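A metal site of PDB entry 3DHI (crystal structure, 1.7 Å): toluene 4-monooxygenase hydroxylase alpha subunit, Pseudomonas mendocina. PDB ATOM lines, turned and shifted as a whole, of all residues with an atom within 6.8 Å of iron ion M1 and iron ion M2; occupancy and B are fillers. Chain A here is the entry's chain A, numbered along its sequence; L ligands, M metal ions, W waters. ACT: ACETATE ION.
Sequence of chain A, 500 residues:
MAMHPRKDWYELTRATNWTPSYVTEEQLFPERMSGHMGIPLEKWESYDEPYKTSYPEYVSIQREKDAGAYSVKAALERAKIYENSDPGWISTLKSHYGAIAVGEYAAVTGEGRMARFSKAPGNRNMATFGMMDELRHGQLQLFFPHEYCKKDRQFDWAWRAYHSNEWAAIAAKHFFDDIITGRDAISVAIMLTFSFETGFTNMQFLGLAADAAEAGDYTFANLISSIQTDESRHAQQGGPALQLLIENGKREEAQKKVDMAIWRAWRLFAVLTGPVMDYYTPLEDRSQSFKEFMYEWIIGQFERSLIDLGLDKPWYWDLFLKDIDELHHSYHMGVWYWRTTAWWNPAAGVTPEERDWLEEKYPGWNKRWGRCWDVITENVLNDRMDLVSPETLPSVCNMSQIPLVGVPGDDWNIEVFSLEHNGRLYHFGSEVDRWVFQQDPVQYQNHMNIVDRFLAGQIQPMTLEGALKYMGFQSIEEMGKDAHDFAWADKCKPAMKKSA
Four residues have an atom within 4 Å of iron ion M2: Glu 134, Glu 197, Glu 231 and His 234.
Iron ion M2 is bound by OE2 of Glu 197 (2.1 Å), OE2 of Glu 134 (2.1 Å), OE2 of Glu 231 (2.1 Å), NE2 of His 234 (2.1 Å), OXT of the ligand (2.2 Å) and OE1 of Glu 231 (2.3 Å).
Slightly farther from iron ion M2 lies an oxygen (O) of the ligand (2.8 Å).
Four residues have an atom within 4 Å of iron ion M1: Glu 104, Glu 134, His 137 and Glu 231.
OE1 of Glu 134 binds iron ion M1.
The side-chain carboxylate (OE2) of Glu 104 is bound to iron ion M1, at 2.1 Å.
Water W1 binds iron ion M1 (2.2 Å).
Iron ion M1 is bound by O of the ligand (2.2 Å).
Iron ion M1 is bound by OE1 of Glu 231, 2.2 Å away.
ND1 of His 137 binds iron ion M1, 2.3 Å away.
The side-chain carboxylate (OE1) of Glu 104 sits close to the side-chain amide oxygen (OE1) of Gln 141 (2.9 Å).
A ring nitrogen (ND1) of His 234 lies within hydrogen-bond range of the side-chain carboxylate (OD2) of Asp 133 (2.7 Å).
OD2 of Asp 230 sits at hydrogen-bond distance from NE2 of His 137, at 2.7 Å.
The side-chain hydroxyl of Thr 201 lies within hydrogen-bond range of the backbone carbonyl oxygen of Glu 197, at 3.2 Å.
The backbone NH of Glu 197 lies within hydrogen-bond range of the backbone carbonyl oxygen of Leu 192, 2.9 Å away.
O of Ile 227 sits at hydrogen-bond distance from NE2 of His 137 (3.4 Å).
The backbone carbonyl oxygen of Asp 230 sits at hydrogen-bond distance from a ring nitrogen (ND1) of His 234.
The side-chain amide oxygen (OE1) of Gln 141 sits close to the backbone carbonyl oxygen (O) of His 137 (3.1 Å).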
ATOM      1  N   GLU A 104     -31.888 -29.106  -5.570  1.00  0.00           N
ATOM      2  CA  GLU A 104     -31.597 -28.712  -6.959  1.00  0.00           C
ATOM      3  C   GLU A 104     -32.821 -28.049  -7.548  1.00  0.00           C
ATOM      4  O   GLU A 104     -32.716 -27.036  -8.194  1.00  0.00           O
ATOM      5  CB  GLU A 104     -31.261 -29.932  -7.843  1.00  0.00           C
ATOM      6  CG  GLU A 104     -29.988 -30.633  -7.466  1.00  0.00           C
ATOM      7  CD  GLU A 104     -28.762 -30.080  -8.164  1.00  0.00           C
ATOM      8  OE1 GLU A 104     -27.755 -30.791  -8.220  1.00  0.00           O
ATOM      9  OE2 GLU A 104     -28.808 -28.931  -8.651  1.00  0.00           O
ATOM     10  N   ALA A 107     -33.098 -24.616  -6.404  1.00  0.00           N
ATOM     11  CA  ALA A 107     -32.150 -23.737  -7.096  1.00  0.00           C
ATOM     12  C   ALA A 107     -32.722 -23.125  -8.366  1.00  0.00           C
ATOM     13  O   ALA A 107     -32.280 -22.058  -8.776  1.00  0.00           O
ATOM     14  CB  ALA A 107     -30.830 -24.472  -7.401  1.00  0.00           C
ATOM     15  N   GLU A 111     -32.223 -19.118  -9.571  1.00  0.00           N
ATOM     16  CA  GLU A 111     -31.952 -18.685 -10.943  1.00  0.00           C
ATOM     17  C   GLU A 111     -33.097 -17.807 -11.450  1.00  0.00           C
ATOM     18  O   GLU A 111     -32.840 -16.774 -12.100  1.00  0.00           O
ATOM     19  CB  GLU A 111     -31.723 -19.881 -11.857  1.00  0.00           C
ATOM     20  CG  GLU A 111     -30.459 -20.695 -11.471  1.00  0.00           C
ATOM     21  CD  GLU A 111     -29.135 -19.989 -11.783  1.00  0.00           C
ATOM     22  OE1 GLU A 111     -29.078 -19.145 -12.697  1.00  0.00           O
ATOM     23  OE2 GLU A 111     -28.107 -20.276 -11.105  1.00  0.00           O
ATOM     24  N   GLY A 130     -29.682 -21.092 -16.477  1.00  0.00           N
ATOM     25  CA  GLY A 130     -29.505 -21.642 -15.109  1.00  0.00           C
ATOM     26  C   GLY A 130     -30.776 -22.291 -14.586  1.00  0.00           C
ATOM     27  O   GLY A 130     -30.741 -23.350 -13.996  1.00  0.00           O
ATOM     28  N   ASP A 133     -30.989 -25.544 -16.311  1.00  0.00           N
ATOM     29  CA  ASP A 133     -29.966 -26.457 -15.757  1.00  0.00           C
ATOM     30  C   ASP A 133     -30.429 -27.084 -14.437  1.00  0.00           C
ATOM     31  O   ASP A 133     -30.275 -28.301 -14.212  1.00  0.00           O
ATOM     32  CB  ASP A 133     -28.654 -25.707 -15.461  1.00  0.00           C
ATOM     33  CG  ASP A 133     -27.893 -25.282 -16.733  1.00  0.00           C
ATOM     34  OD1 ASP A 133     -28.129 -25.819 -17.832  1.00  0.00           O
ATOM     35  OD2 ASP A 133     -27.045 -24.388 -16.608  1.00  0.00           O
ATOM     36  N   GLU A 134     -30.953 -26.254 -13.530  1.00  0.00           N
ATOM     37  CA  GLU A 134     -31.359 -26.799 -12.233  1.00  0.00           C
ATOM     38  C   GLU A 134     -32.596 -27.670 -12.358  1.00  0.00           C
ATOM     39  O   GLU A 134     -32.733 -28.626 -11.598  1.00  0.00           O
ATOM     40  CB  GLU A 134     -31.606 -25.719 -11.204  1.00  0.00           C
ATOM     41  CG  GLU A 134     -30.477 -24.706 -11.046  1.00  0.00           C
ATOM     42  CD  GLU A 134     -29.192 -25.296 -10.489  1.00  0.00           C
ATOM     43  OE1 GLU A 134     -28.976 -26.528 -10.463  1.00  0.00           O
ATOM     44  OE2 GLU A 134     -28.357 -24.479 -10.068  1.00  0.00           O
ATOM     45  N   HIS A 137     -31.172 -30.883 -13.159  1.00  0.00           N
ATOM     46  CA  HIS A 137     -30.487 -31.542 -12.032  1.00  0.00           C
ATOM     47  C   HIS A 137     -31.482 -32.134 -11.055  1.00  0.00           C
ATOM     48  O   HIS A 137     -31.238 -33.224 -10.550  1.00  0.00           O
ATOM     49  CB  HIS A 137     -29.562 -30.567 -11.319  1.00  0.00           C
ATOM     50  CG  HIS A 137     -28.507 -30.007 -12.229  1.00  0.00           C
ATOM     51  ND1 HIS A 137     -27.713 -28.943 -11.873  1.00  0.00           N
ATOM     52  CD2 HIS A 137     -28.130 -30.352 -13.486  1.00  0.00           C
ATOM     53  CE1 HIS A 137     -26.887 -28.658 -12.883  1.00  0.00           C
ATOM     54  NE2 HIS A 137     -27.118 -29.499 -13.870  1.00  0.00           N
ATOM     55  N   GLY A 138     -32.593 -31.426 -10.818  1.00  0.00           N
ATOM     56  CA  GLY A 138     -33.652 -31.955  -9.937  1.00  0.00           C
ATOM     57  C   GLY A 138     -34.278 -33.207 -10.537  1.00  0.00           C
ATOM     58  O   GLY A 138     -34.503 -34.209  -9.835  1.00  0.00           O
ATOM     59  N   GLN A 141     -31.906 -36.229 -10.552  1.00  0.00           N
ATOM     60  CA  GLN A 141     -31.625 -36.742  -9.218  1.00  0.00           C
ATOM     61  C   GLN A 141     -32.869 -37.278  -8.463  1.00  0.00           C
ATOM     62  O   GLN A 141     -32.723 -37.812  -7.372  1.00  0.00           O
ATOM     63  CB  GLN A 141     -30.794 -35.737  -8.419  1.00  0.00           C
ATOM     64  CG  GLN A 141     -29.364 -35.746  -8.962  1.00  0.00           C
ATOM     65  CD  GLN A 141     -28.515 -34.628  -8.459  1.00  0.00           C
ATOM     66  OE1 GLN A 141     -28.804 -33.430  -8.676  1.00  0.00           O
ATOM     67  NE2 GLN A 141     -27.413 -35.004  -7.833  1.00  0.00           N
ATOM     68  N   LEU A 192     -24.827 -17.880  -4.131  1.00  0.00           N
ATOM     69  CA  LEU A 192     -25.096 -19.203  -4.680  1.00  0.00           C
ATOM     70  C   LEU A 192     -24.049 -19.489  -5.745  1.00  0.00           C
ATOM     71  O   LEU A 192     -23.304 -20.449  -5.635  1.00  0.00           O
ATOM     72  CB  LEU A 192     -26.510 -19.315  -5.278  1.00  0.00           C
ATOM     73  CG  LEU A 192     -26.807 -20.515  -6.187  1.00  0.00           C
ATOM     74  CD1 LEU A 192     -26.566 -21.825  -5.462  1.00  0.00           C
ATOM     75  CD2 LEU A 192     -28.277 -20.411  -6.616  1.00  0.00           C
ATOM     76  N   THR A 193     -24.018 -18.646  -6.792  1.00  0.00           N
ATOM     77  CA  THR A 193     -23.321 -19.042  -8.000  1.00  0.00           C
ATOM     78  C   THR A 193     -21.848 -18.878  -7.765  1.00  0.00           C
ATOM     79  O   THR A 193     -21.073 -19.820  -7.953  1.00  0.00           O
ATOM     80  CB  THR A 193     -23.799 -18.313  -9.300  1.00  0.00           C
ATOM     81  OG1 THR A 193     -23.474 -16.930  -9.222  1.00  0.00           O
ATOM     82  CG2 THR A 193     -25.305 -18.476  -9.528  1.00  0.00           C
ATOM     83  N   PHE A 196     -21.170 -20.838  -3.423  1.00  0.00           N
ATOM     84  CA  PHE A 196     -21.529 -22.272  -3.420  1.00  0.00           C
ATOM     85  C   PHE A 196     -21.170 -23.141  -4.673  1.00  0.00           C
ATOM     86  O   PHE A 196     -20.641 -24.255  -4.504  1.00  0.00           O
ATOM     87  CB  PHE A 196     -23.008 -22.436  -3.045  1.00  0.00           C
ATOM     88  CG  PHE A 196     -23.404 -23.840  -2.712  1.00  0.00           C
ATOM     89  CD1 PHE A 196     -22.824 -24.518  -1.654  1.00  0.00           C
ATOM     90  CD2 PHE A 196     -24.396 -24.469  -3.459  1.00  0.00           C
ATOM     91  CE1 PHE A 196     -23.215 -25.806  -1.353  1.00  0.00           C
ATOM     92  CE2 PHE A 196     -24.799 -25.750  -3.159  1.00  0.00           C
ATOM     93  CZ  PHE A 196     -24.208 -26.438  -2.117  1.00  0.00           C
ATOM     94  N   GLU A 197     -21.460 -22.655  -5.879  1.00  0.00           N
ATOM     95  CA  GLU A 197     -21.361 -23.449  -7.122  1.00  0.00           C
ATOM     96  C   GLU A 197     -19.960 -23.542  -7.736  1.00  0.00           C
ATOM     97  O   GLU A 197     -19.725 -24.428  -8.599  1.00  0.00           O
ATOM     98  CB  GLU A 197     -22.319 -22.917  -8.203  1.00  0.00           C
ATOM     99  CG  GLU A 197     -23.770 -22.860  -7.797  1.00  0.00           C
ATOM    100  CD  GLU A 197     -24.651 -22.279  -8.885  1.00  0.00           C
ATOM    101  OE1 GLU A 197     -24.251 -21.297  -9.537  1.00  0.00           O
ATOM    102  OE2 GLU A 197     -25.744 -22.817  -9.116  1.00  0.00           O
ATOM    103  N   THR A 201     -19.695 -27.304  -4.381  1.00  0.00           N
ATOM    104  CA  THR A 201     -20.330 -28.378  -5.158  1.00  0.00           C
ATOM    105  C   THR A 201     -19.300 -29.273  -5.851  1.00  0.00           C
ATOM    106  O   THR A 201     -19.555 -30.467  -6.071  1.00  0.00           O
ATOM    107  CB  THR A 201     -21.384 -27.891  -6.175  1.00  0.00           C
ATOM    108  OG1 THR A 201     -20.783 -26.998  -7.078  1.00  0.00           O
ATOM    109  CG2 THR A 201     -22.526 -27.228  -5.454  1.00  0.00           C
ATOM    110  N   PHE A 205     -19.764 -33.345  -6.073  1.00  0.00           N
ATOM    111  CA  PHE A 205     -20.061 -33.800  -7.401  1.00  0.00           C
ATOM    112  C   PHE A 205     -18.848 -34.226  -8.237  1.00  0.00           C
ATOM    113  O   PHE A 205     -18.996 -34.737  -9.309  1.00  0.00           O
ATOM    114  CB  PHE A 205     -20.834 -32.774  -8.160  1.00  0.00           C
ATOM    115  CG  PHE A 205     -22.240 -32.607  -7.699  1.00  0.00           C
ATOM    116  CD1 PHE A 205     -22.536 -32.044  -6.507  1.00  0.00           C
ATOM    117  CD2 PHE A 205     -23.259 -33.018  -8.472  1.00  0.00           C
ATOM    118  CE1 PHE A 205     -23.831 -31.903  -6.111  1.00  0.00           C
ATOM    119  CE2 PHE A 205     -24.546 -32.879  -8.081  1.00  0.00           C
ATOM    120  CZ  PHE A 205     -24.821 -32.307  -6.880  1.00  0.00           C
ATOM    121  N   ILE A 227     -23.660 -33.437 -14.366  1.00  0.00           N
ATOM    122  CA  ILE A 227     -24.338 -32.335 -13.711  1.00  0.00           C
ATOM    123  C   ILE A 227     -23.392 -31.163 -13.474  1.00  0.00           C
ATOM    124  O   ILE A 227     -23.723 -30.002 -13.742  1.00  0.00           O
ATOM    125  CB  ILE A 227     -24.963 -32.832 -12.396  1.00  0.00           C
ATOM    126  CG1 ILE A 227     -26.191 -33.696 -12.729  1.00  0.00           C
ATOM    127  CG2 ILE A 227     -25.336 -31.661 -11.502  1.00  0.00           C
ATOM    128  CD1 ILE A 227     -26.908 -34.294 -11.533  1.00  0.00           C
ATOM    129  N   GLN A 228     -22.169 -31.465 -13.036  1.00  0.00           N
ATOM    130  CA  GLN A 228     -21.221 -30.407 -12.709  1.00  0.00           C
ATOM    131  C   GLN A 228     -20.780 -29.568 -13.930  1.00  0.00           C
ATOM    132  O   GLN A 228     -20.393 -28.409 -13.780  1.00  0.00           O
ATOM    133  CB  GLN A 228     -20.026 -30.960 -11.944  1.00  0.00           C
ATOM    134  CG  GLN A 228     -19.315 -29.888 -11.099  1.00  0.00           C
ATOM    135  CD  GLN A 228     -20.177 -29.334  -9.971  1.00  0.00           C
ATOM    136  OE1 GLN A 228     -21.342 -29.738  -9.771  1.00  0.00           O
ATOM    137  NE2 GLN A 228     -19.606 -28.397  -9.202  1.00  0.00           N
ATOM    138  N   ASP A 230     -22.750 -28.431 -16.128  1.00  0.00           N
ATOM    139  CA  ASP A 230     -23.712 -27.302 -16.188  1.00  0.00           C
ATOM    140  C   ASP A 230     -23.382 -26.258 -15.141  1.00  0.00           C
ATOM    141  O   ASP A 230     -23.427 -25.052 -15.387  1.00  0.00           O
ATOM    142  CB  ASP A 230     -25.145 -27.778 -15.912  1.00  0.00           C
ATOM    143  CG  ASP A 230     -25.644 -28.798 -16.904  1.00  0.00           C
ATOM    144  OD1 ASP A 230     -25.305 -28.709 -18.106  1.00  0.00           O
ATOM    145  OD2 ASP A 230     -26.431 -29.696 -16.479  1.00  0.00           O
ATOM    146  N   GLU A 231     -23.076 -26.729 -13.932  1.00  0.00           N
ATOM    147  CA  GLU A 231     -22.749 -25.837 -12.812  1.00  0.00           C
ATOM    148  C   GLU A 231     -21.587 -24.969 -13.234  1.00  0.00           C
ATOM    149  O   GLU A 231     -21.580 -23.764 -12.995  1.00  0.00           O
ATOM    150  CB  GLU A 231     -22.348 -26.649 -11.582  1.00  0.00           C
ATOM    151  CG  GLU A 231     -23.554 -27.399 -10.938  1.00  0.00           C
ATOM    152  CD  GLU A 231     -24.641 -26.444 -10.482  1.00  0.00           C
ATOM    153  OE1 GLU A 231     -25.840 -26.693 -10.789  1.00  0.00           O
ATOM    154  OE2 GLU A 231     -24.332 -25.385  -9.883  1.00  0.00           O
ATOM    155  N   HIS A 234     -23.115 -22.107 -15.495  1.00  0.00           N
ATOM    156  CA  HIS A 234     -23.999 -21.097 -14.880  1.00  0.00           C
ATOM    157  C   HIS A 234     -23.417 -20.428 -13.631  1.00  0.00           C
ATOM    158  O   HIS A 234     -23.810 -19.304 -13.255  1.00  0.00           O
ATOM    159  CB  HIS A 234     -25.461 -21.566 -14.727  1.00  0.00           C
ATOM    160  CG  HIS A 234     -25.700 -22.640 -13.696  1.00  0.00           C
ATOM    161  ND1 HIS A 234     -26.310 -23.835 -14.018  1.00  0.00           N
ATOM    162  CD2 HIS A 234     -25.523 -22.656 -12.357  1.00  0.00           C
ATOM    163  CE1 HIS A 234     -26.445 -24.568 -12.928  1.00  0.00           C
ATOM    164  NE2 HIS A 234     -25.989 -23.873 -11.901  1.00  0.00           N
ATOM    165  N   ALA A 235     -22.460 -21.093 -12.977  1.00  0.00           N
ATOM    166  CA  ALA A 235     -21.768 -20.486 -11.839  1.00  0.00           C
ATOM    167  C   ALA A 235     -20.996 -19.217 -12.234  1.00  0.00           C
ATOM    168  O   ALA A 235     -20.697 -18.373 -11.391  1.00  0.00           O
ATOM    169  CB  ALA A 235     -20.839 -21.494 -11.176  1.00  0.00           C
HETATM  170  C   ACT L   1     -26.941 -25.744  -7.263  1.00  0.00           C
HETATM  171  O   ACT L   1     -27.107 -26.627  -8.122  1.00  0.00           O
HETATM  172  OXT ACT L   1     -26.480 -24.674  -7.698  1.00  0.00           O
HETATM  173  CH3 ACT L   1     -27.293 -25.941  -5.823  1.00  0.00           C
HETATM  174 FE    FE M   1     -27.491 -27.859  -9.908  1.00  0.00          FE
HETATM  175 FE    FE M   2     -26.298 -24.628  -9.919  1.00  0.00          FE
HETATM  176  O   HOH W   1     -25.967 -29.255  -9.154  1.00  0.00           O
